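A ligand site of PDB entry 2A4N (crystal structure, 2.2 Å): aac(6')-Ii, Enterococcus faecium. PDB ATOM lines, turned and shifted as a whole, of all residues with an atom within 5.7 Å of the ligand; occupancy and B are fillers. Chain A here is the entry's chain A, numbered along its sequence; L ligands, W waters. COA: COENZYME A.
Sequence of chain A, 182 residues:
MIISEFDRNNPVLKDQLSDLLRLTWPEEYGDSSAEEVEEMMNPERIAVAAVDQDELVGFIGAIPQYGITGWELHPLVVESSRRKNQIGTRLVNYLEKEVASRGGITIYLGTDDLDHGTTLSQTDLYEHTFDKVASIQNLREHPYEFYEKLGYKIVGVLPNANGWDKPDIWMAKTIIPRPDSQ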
ATOM      1  N   TRP A  25      -8.942  23.130 -41.068  1.00  0.00           N
ATOM      2  CA  TRP A  25      -9.536  22.452 -42.215  1.00  0.00           C
ATOM      3  C   TRP A  25      -9.462  23.333 -43.459  1.00  0.00           C
ATOM      4  O   TRP A  25     -10.476  23.823 -43.944  1.00  0.00           O
ATOM      5  CD2 TRP A  25     -11.675  21.329 -39.503  1.00  0.00           C
ATOM      6  NE1 TRP A  25     -11.082  19.168 -39.665  1.00  0.00           N
ATOM      7  CE2 TRP A  25     -11.613  20.100 -38.816  1.00  0.00           C
ATOM      8  CZ3 TRP A  25     -12.627  22.307 -37.531  1.00  0.00           C
ATOM      9  N   LEU A  76     -16.235  21.817 -33.907  1.00  0.00           N
ATOM     10  CA  LEU A  76     -15.545  21.864 -32.626  1.00  0.00           C
ATOM     11  C   LEU A  76     -14.070  21.990 -32.949  1.00  0.00           C
ATOM     12  O   LEU A  76     -13.490  21.119 -33.611  1.00  0.00           O
ATOM     13  CB  LEU A  76     -15.790  20.604 -31.794  1.00  0.00           C
ATOM     14  CG  LEU A  76     -14.959  20.482 -30.514  1.00  0.00           C
ATOM     15  CD1 LEU A  76     -15.098  21.733 -29.651  1.00  0.00           C
ATOM     16  CD2 LEU A  76     -15.412  19.251 -29.747  1.00  0.00           C
ATOM     17  N   VAL A  77     -13.466  23.076 -32.503  1.00  0.00           N
ATOM     18  CA  VAL A  77     -12.055  23.321 -32.755  1.00  0.00           C
ATOM     19  C   VAL A  77     -11.389  24.055 -31.600  1.00  0.00           C
ATOM     20  O   VAL A  77     -11.940  25.004 -31.047  1.00  0.00           O
ATOM     21  CB  VAL A  77     -11.864  24.153 -34.046  1.00  0.00           C
ATOM     22  CG1 VAL A  77     -12.557  25.501 -33.902  1.00  0.00           C
ATOM     23  CG2 VAL A  77     -10.395  24.335 -34.326  1.00  0.00           C
ATOM     24  N   VAL A  78     -10.206  23.588 -31.238  1.00  0.00           N
ATOM     25  CA  VAL A  78      -9.409  24.196 -30.182  1.00  0.00           C
ATOM     26  C   VAL A  78      -8.046  24.451 -30.821  1.00  0.00           C
ATOM     27  O   VAL A  78      -7.541  23.588 -31.525  1.00  0.00           O
ATOM     28  CB  VAL A  78      -9.217  23.224 -28.987  1.00  0.00           C
ATOM     29  CG1 VAL A  78      -8.245  23.826 -27.985  1.00  0.00           C
ATOM     30  CG2 VAL A  78     -10.557  22.933 -28.316  1.00  0.00           C
ATOM     31  N   GLU A  79      -7.485  25.638 -30.596  1.00  0.00           N
ATOM     32  CA  GLU A  79      -6.176  25.950 -31.172  1.00  0.00           C
ATOM     33  C   GLU A  79      -5.206  24.811 -30.844  1.00  0.00           C
ATOM     34  O   GLU A  79      -5.194  24.306 -29.727  1.00  0.00           O
ATOM     35  CB  GLU A  79      -5.630  27.254 -30.597  1.00  0.00           C
ATOM     36  OE2 GLU A  79      -5.326  30.571 -31.381  1.00  0.00           O
ATOM     37  N   ARG A  82      -3.263  25.036 -27.774  1.00  0.00           N
ATOM     38  CA  ARG A  82      -4.023  25.031 -26.526  1.00  0.00           C
ATOM     39  C   ARG A  82      -4.781  23.733 -26.298  1.00  0.00           C
ATOM     40  O   ARG A  82      -5.681  23.682 -25.455  1.00  0.00           O
ATOM     41  CB  ARG A  82      -4.999  26.202 -26.504  1.00  0.00           C
ATOM     42  CD  ARG A  82      -3.840  27.726 -24.909  1.00  0.00           C
ATOM     43  NE  ARG A  82      -3.172  29.012 -24.723  1.00  0.00           N
ATOM     44  CZ  ARG A  82      -3.779  30.186 -24.837  1.00  0.00           C
ATOM     45  N   ARG A  83      -4.440  22.687 -27.044  1.00  0.00           N
ATOM     46  CA  ARG A  83      -5.117  21.411 -26.916  1.00  0.00           C
ATOM     47  C   ARG A  83      -4.635  20.582 -25.735  1.00  0.00           C
ATOM     48  O   ARG A  83      -3.665  20.939 -25.068  1.00  0.00           O
ATOM     49  CB  ARG A  83      -4.972  20.610 -28.209  1.00  0.00           C
ATOM     50  CG  ARG A  83      -5.703  21.240 -29.382  1.00  0.00           C
ATOM     51  CD  ARG A  83      -5.508  20.460 -30.673  1.00  0.00           C
ATOM     52  NE  ARG A  83      -6.065  21.175 -31.805  1.00  0.00           N
ATOM     53  CZ  ARG A  83      -5.859  20.861 -33.079  1.00  0.00           C
ATOM     54  NH1 ARG A  83      -5.093  19.826 -33.384  1.00  0.00           N
ATOM     55  NH2 ARG A  83      -6.409  21.590 -34.042  1.00  0.00           N
ATOM     56  N   LYS A  84      -5.331  19.468 -25.483  1.00  0.00           N
ATOM     57  CA  LYS A  84      -5.007  18.576 -24.378  1.00  0.00           C
ATOM     58  C   LYS A  84      -4.918  19.342 -23.059  1.00  0.00           C
ATOM     59  O   LYS A  84      -4.079  19.033 -22.214  1.00  0.00           O
ATOM     60  CB  LYS A  84      -3.695  17.831 -24.643  1.00  0.00           C
ATOM     61  CG  LYS A  84      -3.766  16.836 -25.795  1.00  0.00           C
ATOM     62  N   ASN A  85      -5.789  20.336 -22.900  1.00  0.00           N
ATOM     63  CA  ASN A  85      -5.823  21.160 -21.696  1.00  0.00           C
ATOM     64  C   ASN A  85      -7.255  21.280 -21.140  1.00  0.00           C
ATOM     65  O   ASN A  85      -7.507  22.035 -20.214  1.00  0.00           O
ATOM     66  CB  ASN A  85      -5.273  22.557 -21.988  1.00  0.00           C
ATOM     67  CG  ASN A  85      -5.018  23.374 -20.720  1.00  0.00           C
ATOM     68  OD1 ASN A  85      -4.837  24.584 -20.778  1.00  0.00           O
ATOM     69  ND2 ASN A  85      -5.013  22.700 -19.575  1.00  0.00           N
ATOM     70  N   GLN A  86      -8.177  20.534 -21.737  1.00  0.00           N
ATOM     71  CA  GLN A  86      -9.582  20.520 -21.320  1.00  0.00           C
ATOM     72  C   GLN A  86     -10.473  21.648 -21.855  1.00  0.00           C
ATOM     73  O   GLN A  86     -11.580  21.853 -21.359  1.00  0.00           O
ATOM     74  CB  GLN A  86      -9.660  20.486 -19.785  1.00  0.00           C
ATOM     75  CG  GLN A  86      -9.092  19.216 -19.163  1.00  0.00           C
ATOM     76  CD  GLN A  86     -10.012  18.021 -19.344  1.00  0.00           C
ATOM     77  N   ILE A  87     -10.002  22.364 -22.862  1.00  0.00           N
ATOM     78  CA  ILE A  87     -10.827  23.421 -23.446  1.00  0.00           C
ATOM     79  C   ILE A  87     -11.985  22.768 -24.196  1.00  0.00           C
ATOM     80  O   ILE A  87     -13.127  23.246 -24.149  1.00  0.00           O
ATOM     81  CB  ILE A  87     -10.002  24.273 -24.424  1.00  0.00           C
ATOM     82  CG1 ILE A  87      -8.892  25.004 -23.647  1.00  0.00           C
ATOM     83  CG2 ILE A  87     -10.922  25.260 -25.155  1.00  0.00           C
ATOM     84  CD1 ILE A  87      -7.896  25.734 -24.522  1.00  0.00           C
ATOM     85  N   GLY A  88     -11.689  21.671 -24.888  1.00  0.00           N
ATOM     86  CA  GLY A  88     -12.724  20.961 -25.609  1.00  0.00           C
ATOM     87  C   GLY A  88     -13.803  20.470 -24.653  1.00  0.00           C
ATOM     88  O   GLY A  88     -14.992  20.689 -24.881  1.00  0.00           O
ATOM     89  N   THR A  89     -13.381  19.825 -23.563  1.00  0.00           N
ATOM     90  CA  THR A  89     -14.305  19.305 -22.566  1.00  0.00           C
ATOM     91  C   THR A  89     -15.257  20.396 -22.099  1.00  0.00           C
ATOM     92  O   THR A  89     -16.479  20.195 -22.065  1.00  0.00           O
ATOM     93  CB  THR A  89     -13.548  18.745 -21.338  1.00  0.00           C
ATOM     94  OG1 THR A  89     -12.740  17.625 -21.733  1.00  0.00           O
ATOM     95  CG2 THR A  89     -14.526  18.288 -20.271  1.00  0.00           C
ATOM     96  N   ARG A  90     -14.693  21.539 -21.748  1.00  0.00           N
ATOM     97  CA  ARG A  90     -15.493  22.665 -21.275  1.00  0.00           C
ATOM     98  C   ARG A  90     -16.425  23.217 -22.350  1.00  0.00           C
ATOM     99  O   ARG A  90     -17.512  23.686 -22.047  1.00  0.00           O
ATOM    100  CB  ARG A  90     -14.568  23.751 -20.733  1.00  0.00           C
ATOM    101  CG  ARG A  90     -13.754  23.248 -19.539  1.00  0.00           C
ATOM    102  CD  ARG A  90     -12.372  23.865 -19.465  1.00  0.00           C
ATOM    103  NE  ARG A  90     -12.379  25.204 -18.899  1.00  0.00           N
ATOM    104  CZ  ARG A  90     -11.326  26.005 -18.891  1.00  0.00           C
ATOM    105  NH1 ARG A  90     -10.182  25.609 -19.427  1.00  0.00           N
ATOM    106  NH2 ARG A  90     -11.424  27.202 -18.331  1.00  0.00           N
ATOM    107  N   LEU A 109     -23.047  13.798 -33.822  1.00  0.00           N
ATOM    108  CA  LEU A 109     -22.019  14.351 -34.680  1.00  0.00           C
ATOM    109  C   LEU A 109     -21.463  13.264 -35.590  1.00  0.00           C
ATOM    110  O   LEU A 109     -21.679  12.074 -35.365  1.00  0.00           O
ATOM    111  CB  LEU A 109     -20.881  14.941 -33.836  1.00  0.00           C
ATOM    112  CG  LEU A 109     -20.293  13.978 -32.801  1.00  0.00           C
ATOM    113  CD1 LEU A 109     -19.136  13.187 -33.413  1.00  0.00           C
ATOM    114  CD2 LEU A 109     -19.802  14.747 -31.579  1.00  0.00           C
ATOM    115  N   GLY A 110     -20.753  13.706 -36.617  1.00  0.00           N
ATOM    116  CA  GLY A 110     -20.119  12.803 -37.547  1.00  0.00           C
ATOM    117  C   GLY A 110     -18.634  13.117 -37.564  1.00  0.00           C
ATOM    118  O   GLY A 110     -18.239  14.203 -38.000  1.00  0.00           O
ATOM    119  N   THR A 111     -17.819  12.195 -37.070  1.00  0.00           N
ATOM    120  CA  THR A 111     -16.382  12.396 -37.070  1.00  0.00           C
ATOM    121  C   THR A 111     -15.815  11.487 -38.157  1.00  0.00           C
ATOM    122  O   THR A 111     -15.924  10.263 -38.078  1.00  0.00           O
ATOM    123  CB  THR A 111     -15.741  12.074 -35.686  1.00  0.00           C
ATOM    124  OG1 THR A 111     -14.322  12.255 -35.762  1.00  0.00           O
ATOM    125  CG2 THR A 111     -16.056  10.656 -35.255  1.00  0.00           C
ATOM    126  N   ASP A 112     -15.225  12.084 -39.184  1.00  0.00           N
ATOM    127  CA  ASP A 112     -14.680  11.324 -40.289  1.00  0.00           C
ATOM    128  C   ASP A 112     -13.316  10.702 -40.032  1.00  0.00           C
ATOM    129  O   ASP A 112     -12.510  11.242 -39.291  1.00  0.00           O
ATOM    130  CB  ASP A 112     -14.606  12.197 -41.540  1.00  0.00           C
ATOM    131  CG  ASP A 112     -15.917  12.862 -41.873  1.00  0.00           C
ATOM    132  OD1 ASP A 112     -16.265  13.853 -41.198  1.00  0.00           O
ATOM    133  OD2 ASP A 112     -16.600  12.395 -42.797  1.00  0.00           O
ATOM    134  N   ASN A 138      -8.467   2.937 -31.320  1.00  0.00           N
ATOM    135  CA  ASN A 138      -7.906   4.193 -31.799  1.00  0.00           C
ATOM    136  C   ASN A 138      -6.460   3.960 -32.229  1.00  0.00           C
ATOM    137  O   ASN A 138      -5.605   3.587 -31.422  1.00  0.00           O
ATOM    138  CB  ASN A 138      -7.938   5.252 -30.686  1.00  0.00           C
ATOM    139  CG  ASN A 138      -7.816   6.664 -31.233  1.00  0.00           C
ATOM    140  OD1 ASN A 138      -7.440   6.851 -32.399  1.00  0.00           O
ATOM    141  ND2 ASN A 138      -8.108   7.653 -30.407  1.00  0.00           N
ATOM    142  N   GLU A 141      -4.628   8.526 -32.466  1.00  0.00           N
ATOM    143  CA  GLU A 141      -5.274   9.558 -31.661  1.00  0.00           C
ATOM    144  C   GLU A 141      -6.437  10.198 -32.421  1.00  0.00           C
ATOM    145  O   GLU A 141      -6.495  11.423 -32.569  1.00  0.00           O
ATOM    146  CB  GLU A 141      -4.262  10.631 -31.255  1.00  0.00           C
ATOM    147  CG  GLU A 141      -3.085  10.096 -30.446  1.00  0.00           C
ATOM    148  CD  GLU A 141      -2.241  11.203 -29.817  1.00  0.00           C
ATOM    149  OE1 GLU A 141      -1.806  12.115 -30.564  1.00  0.00           O
ATOM    150  OE2 GLU A 141      -1.999  11.143 -28.598  1.00  0.00           O
ATOM    151  N   HIS A 142      -7.338   9.366 -32.921  1.00  0.00           N
ATOM    152  CA  HIS A 142      -8.505   9.879 -33.625  1.00  0.00           C
ATOM    153  C   HIS A 142      -9.398  10.519 -32.579  1.00  0.00           C
ATOM    154  O   HIS A 142      -9.537   9.993 -31.468  1.00  0.00           O
ATOM    155  CB  HIS A 142      -9.274   8.752 -34.311  1.00  0.00           C
ATOM    156  CG  HIS A 142     -10.396   9.245 -35.169  1.00  0.00           C
ATOM    157  ND1 HIS A 142     -10.194   9.695 -36.464  1.00  0.00           N
ATOM    158  CD2 HIS A 142     -11.708   9.410 -34.923  1.00  0.00           C
ATOM    159  CE1 HIS A 142     -11.341  10.114 -36.965  1.00  0.00           C
ATOM    160  NE2 HIS A 142     -12.283   9.956 -36.041  1.00  0.00           N
ATOM    161  N   PRO A 143     -10.017  11.659 -32.913  1.00  0.00           N
ATOM    162  CA  PRO A 143     -10.901  12.371 -31.980  1.00  0.00           C
ATOM    163  C   PRO A 143     -12.191  11.685 -31.530  1.00  0.00           C
ATOM    164  O   PRO A 143     -12.867  12.185 -30.635  1.00  0.00           O
ATOM    165  CB  PRO A 143     -11.149  13.692 -32.712  1.00  0.00           C
ATOM    166  CG  PRO A 143     -11.101  13.273 -34.163  1.00  0.00           C
ATOM    167  CD  PRO A 143      -9.906  12.377 -34.197  1.00  0.00           C
ATOM    168  N   GLU A 145     -12.467   9.139 -29.833  1.00  0.00           N
ATOM    169  CA  GLU A 145     -12.209   8.739 -28.462  1.00  0.00           C
ATOM    170  C   GLU A 145     -12.408   9.904 -27.495  1.00  0.00           C
ATOM    171  O   GLU A 145     -12.784   9.709 -26.336  1.00  0.00           O
ATOM    172  CB  GLU A 145     -10.800   8.161 -28.351  1.00  0.00           C
ATOM    173  CG  GLU A 145     -10.503   7.506 -27.001  1.00  0.00           C
ATOM    174  CD  GLU A 145      -9.364   6.512 -27.101  1.00  0.00           C
ATOM    175  OE1 GLU A 145      -8.289   6.879 -27.596  1.00  0.00           O
ATOM    176  OE2 GLU A 145      -9.549   5.349 -26.666  1.00  0.00           O
ATOM    177  N   PHE A 146     -12.167  11.118 -27.970  1.00  0.00           N
ATOM    178  CA  PHE A 146     -12.360  12.305 -27.152  1.00  0.00           C
ATOM    179  C   PHE A 146     -13.831  12.356 -26.778  1.00  0.00           C
ATOM    180  O   PHE A 146     -14.187  12.543 -25.604  1.00  0.00           O
ATOM    181  CB  PHE A 146     -12.021  13.564 -27.950  1.00  0.00           C
ATOM    182  CG  PHE A 146     -12.600  14.831 -27.370  1.00  0.00           C
ATOM    183  CD1 PHE A 146     -12.120  15.345 -26.163  1.00  0.00           C
ATOM    184  CD2 PHE A 146     -13.632  15.499 -28.030  1.00  0.00           C
ATOM    185  CE1 PHE A 146     -12.661  16.513 -25.616  1.00  0.00           C
ATOM    186  CE2 PHE A 146     -14.185  16.675 -27.489  1.00  0.00           C
ATOM    187  CZ  PHE A 146     -13.694  17.174 -26.283  1.00  0.00           C
ATOM    188  N   TYR A 147     -14.684  12.172 -27.782  1.00  0.00           N
ATOM    189  CA  TYR A 147     -16.120  12.209 -27.568  1.00  0.00           C
ATOM    190  C   TYR A 147     -16.600  11.062 -26.670  1.00  0.00           C
ATOM    191  O   TYR A 147     -17.483  11.266 -25.841  1.00  0.00           O
ATOM    192  CB  TYR A 147     -16.847  12.191 -28.917  1.00  0.00           C
ATOM    193  CG  TYR A 147     -16.628  13.464 -29.717  1.00  0.00           C
ATOM    194  CD1 TYR A 147     -17.235  14.662 -29.319  1.00  0.00           C
ATOM    195  CD2 TYR A 147     -15.816  13.483 -30.842  1.00  0.00           C
ATOM    196  CE1 TYR A 147     -17.041  15.842 -30.054  1.00  0.00           C
ATOM    197  CE2 TYR A 147     -15.610  14.649 -31.564  1.00  0.00           C
ATOM    198  CZ  TYR A 147     -16.217  15.825 -31.173  1.00  0.00           C
ATOM    199  OH  TYR A 147     -16.000  16.984 -31.889  1.00  0.00           O
ATOM    200  N   LYS A 149     -15.054   9.680 -24.199  1.00  0.00           N
ATOM    201  CA  LYS A 149     -14.727  10.057 -22.828  1.00  0.00           C
ATOM    202  C   LYS A 149     -15.679  11.090 -22.263  1.00  0.00           C
ATOM    203  O   LYS A 149     -15.799  11.207 -21.042  1.00  0.00           O
ATOM    204  CB  LYS A 149     -13.283  10.540 -22.740  1.00  0.00           C
ATOM    205  CG  LYS A 149     -12.273   9.391 -22.829  1.00  0.00           C
ATOM    206  CD  LYS A 149     -10.816   9.874 -22.814  1.00  0.00           C
ATOM    207  CE  LYS A 149      -9.867   8.688 -22.804  1.00  0.00           C
ATOM    208  NZ  LYS A 149      -8.430   9.081 -22.894  1.00  0.00           N
ATOM    209  N   LEU A 150     -16.360  11.832 -23.127  1.00  0.00           N
ATOM    210  CA  LEU A 150     -17.321  12.823 -22.661  1.00  0.00           C
ATOM    211  C   LEU A 150     -18.727  12.240 -22.668  1.00  0.00           C
ATOM    212  O   LEU A 150     -19.713  12.966 -22.556  1.00  0.00           O
ATOM    213  CB  LEU A 150     -17.270  14.089 -23.522  1.00  0.00           C
ATOM    214  CG  LEU A 150     -16.004  14.953 -23.399  1.00  0.00           C
ATOM    215  CD1 LEU A 150     -16.150  16.204 -24.227  1.00  0.00           C
ATOM    216  CD2 LEU A 150     -15.779  15.309 -21.941  1.00  0.00           C
HETATM  217  N1A COA L   1      -7.630  11.031 -29.240  1.00  0.00           N
HETATM  218  C2A COA L   1      -7.832  10.434 -28.052  1.00  0.00           C
HETATM  219  N3A COA L   1      -8.140  11.010 -26.887  1.00  0.00           N
HETATM  220  C4A COA L   1      -8.246  12.376 -27.014  1.00  0.00           C
HETATM  221  C5A COA L   1      -8.071  13.121 -28.162  1.00  0.00           C
HETATM  222  C6A COA L   1      -7.745  12.390 -29.345  1.00  0.00           C
HETATM  223  N6A COA L   1      -7.542  12.973 -30.519  1.00  0.00           N
HETATM  224  N7A COA L   1      -8.259  14.462 -27.891  1.00  0.00           N
HETATM  225  C8A COA L   1      -8.546  14.501 -26.633  1.00  0.00           C
HETATM  226  N9A COA L   1      -8.552  13.265 -26.017  1.00  0.00           N
HETATM  227  C1B COA L   1      -8.833  12.927 -24.613  1.00  0.00           C
HETATM  228  C2B COA L   1      -7.833  13.536 -23.635  1.00  0.00           C
HETATM  229  O2B COA L   1      -6.731  12.639 -23.489  1.00  0.00           O
HETATM  230  C3B COA L   1      -8.575  13.643 -22.302  1.00  0.00           C
HETATM  231  O3B COA L   1      -8.600  12.351 -21.685  1.00  0.00           O
HETATM  232  P3B COA L   1      -7.857  12.086 -20.283  1.00  0.00           P
HETATM  233  O7A COA L   1      -6.483  12.593 -20.494  1.00  0.00           O
HETATM  234  O8A COA L   1      -7.947  10.614 -20.116  1.00  0.00           O
HETATM  235  O9A COA L   1      -8.667  12.861 -19.308  1.00  0.00           O
HETATM  236  C4B COA L   1     -10.009  13.956 -22.768  1.00  0.00           C
HETATM  237  O4B COA L   1     -10.069  13.422 -24.095  1.00  0.00           O
HETATM  238  C5B COA L   1     -10.353  15.454 -22.749  1.00  0.00           C
HETATM  239  O5B COA L   1      -9.492  16.128 -23.668  1.00  0.00           O
HETATM  240  P1A COA L   1      -9.495  17.721 -23.861  1.00  0.00           P
HETATM  241  O1A COA L   1     -10.786  18.266 -23.386  1.00  0.00           O
HETATM  242  O2A COA L   1      -8.227  18.249 -23.322  1.00  0.00           O
HETATM  243  O3A COA L   1      -9.454  17.812 -25.463  1.00  0.00           O
HETATM  244  P2A COA L   1      -9.040  19.114 -26.310  1.00  0.00           P
HETATM  245  O4A COA L   1      -7.688  18.881 -26.873  1.00  0.00           O
HETATM  246  O5A COA L   1      -9.304  20.316 -25.500  1.00  0.00           O
HETATM  247  O6A COA L   1     -10.105  19.094 -27.526  1.00  0.00           O
HETATM  248  CBP COA L   1     -10.394  18.123 -29.751  1.00  0.00           C
HETATM  249  CCP COA L   1     -10.365  17.884 -28.250  1.00  0.00           C
HETATM  250  CDP COA L   1     -10.511  16.771 -30.461  1.00  0.00           C
HETATM  251  CEP COA L   1     -11.638  19.000 -30.103  1.00  0.00           C
HETATM  252  CAP COA L   1      -9.030  18.857 -30.158  1.00  0.00           C
HETATM  253  OAP COA L   1      -7.897  17.996 -30.008  1.00  0.00           O
HETATM  254  C9P COA L   1      -9.072  19.470 -31.577  1.00  0.00           C
HETATM  255  O9P COA L   1      -9.311  20.680 -31.721  1.00  0.00           O
HETATM  256  N8P COA L   1      -8.829  18.631 -32.589  1.00  0.00           N
HETATM  257  C7P COA L   1      -8.810  18.990 -34.002  1.00  0.00           C
HETATM  258  C6P COA L   1     -10.204  19.211 -34.579  1.00  0.00           C
HETATM  259  C5P COA L   1     -11.075  17.958 -34.581  1.00  0.00           C
HETATM  260  O5P COA L   1     -10.663  16.916 -35.114  1.00  0.00           O
HETATM  261  N4P COA L   1     -12.273  18.070 -33.985  1.00  0.00           N
HETATM  262  C3P COA L   1     -13.263  16.992 -33.867  1.00  0.00           C
HETATM  263  C2P COA L   1     -14.469  17.210 -34.768  1.00  0.00           C
HETATM  264  S1P COA L   1     -14.901  15.732 -35.718  1.00  0.00           S
HETATM  265  O   HOH W   1      -7.788  22.163 -24.455  1.00  0.00           O
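N1A of the ligand sits close to O of His 142, at 3.1 Å. Merely in contact with the ligand: Val 77 (3.9 Å), Asn 138 (3.6 Å), Pro 143 (3.7 Å), Glu 145 (3.6 Å), Phe 146 (3.4 Å) and Tyr 147 (3.3 Å). Hydrophobic or aromatic side chains that line the ligand: Leu 76, Val 78, Pro 143 and Phe 146. The nearest printed residue that does not touch the ligand is Gly 110 (4.3 Å).
The side-chain hydroxyl of Thr 111 sits close to a sulfur (S1P) of the ligand, at 3.5 Å. An oxygen (O5A) of the ligand lies within hydrogen-bond range of the backbone NH of Ile 87, 3.4 Å away. An oxygen (O9P) of the ligand is in hydrogen-bond range of the guanidinium group (NE) of Arg 83, 3.3 Å away. O of Leu 76 is in hydrogen-bond range of N4P of the ligand (3.3 Å). N of Val 78 sits at hydrogen-bond distance from O9P of the ligand (3.1 Å). OG1 of Thr 89 lies within hydrogen-bond range of O1A of the ligand (2.6 Å). N of Asn 85 is in hydrogen-bond range of O2A of the ligand (3.2 Å). The side-chain amino group (NZ) of Lys 149 is in salt-bridge range of an oxygen (O8A) of the ligand (3.2 Å). The backbone NH (N) of Thr 89 is in hydrogen-bond range of an oxygen (O1A) of the ligand (3.0 Å). The backbone NH (N) of Gln 86 lies within hydrogen-bond range of an oxygen (O2A) of the ligand. The backbone NH of Gly 88 lies within hydrogen-bond range of an oxygen (O5A) of the ligand (2.8 Å). A nitrogen (N6A) of the ligand sits at hydrogen-bond distance from the backbone carbonyl oxygen (O) of Glu 141. An oxygen (O4A) of the ligand is in hydrogen-bond range of the backbone NH (N) of Lys 84.
The backbone NH (N) of His 142 lies within hydrogen-bond range of the side-chain amide oxygen (OD1) of Asn 138 (2.6 Å). OD1 of Asn 138 is in hydrogen-bond range of N of Glu 141 (3.3 Å). The guanidinium group (NE) of Arg 83 sits at hydrogen-bond distance from the backbone carbonyl oxygen (O) of Val 78, at 2.8 Å. A ring nitrogen (NE2) of His 142 lies within hydrogen-bond range of the side-chain hydroxyl (OG1) of Thr 111, at 3.1 Å. ND2 of Asn 138 sits at hydrogen-bond distance from OE1 of Glu 145 (2.9 Å).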
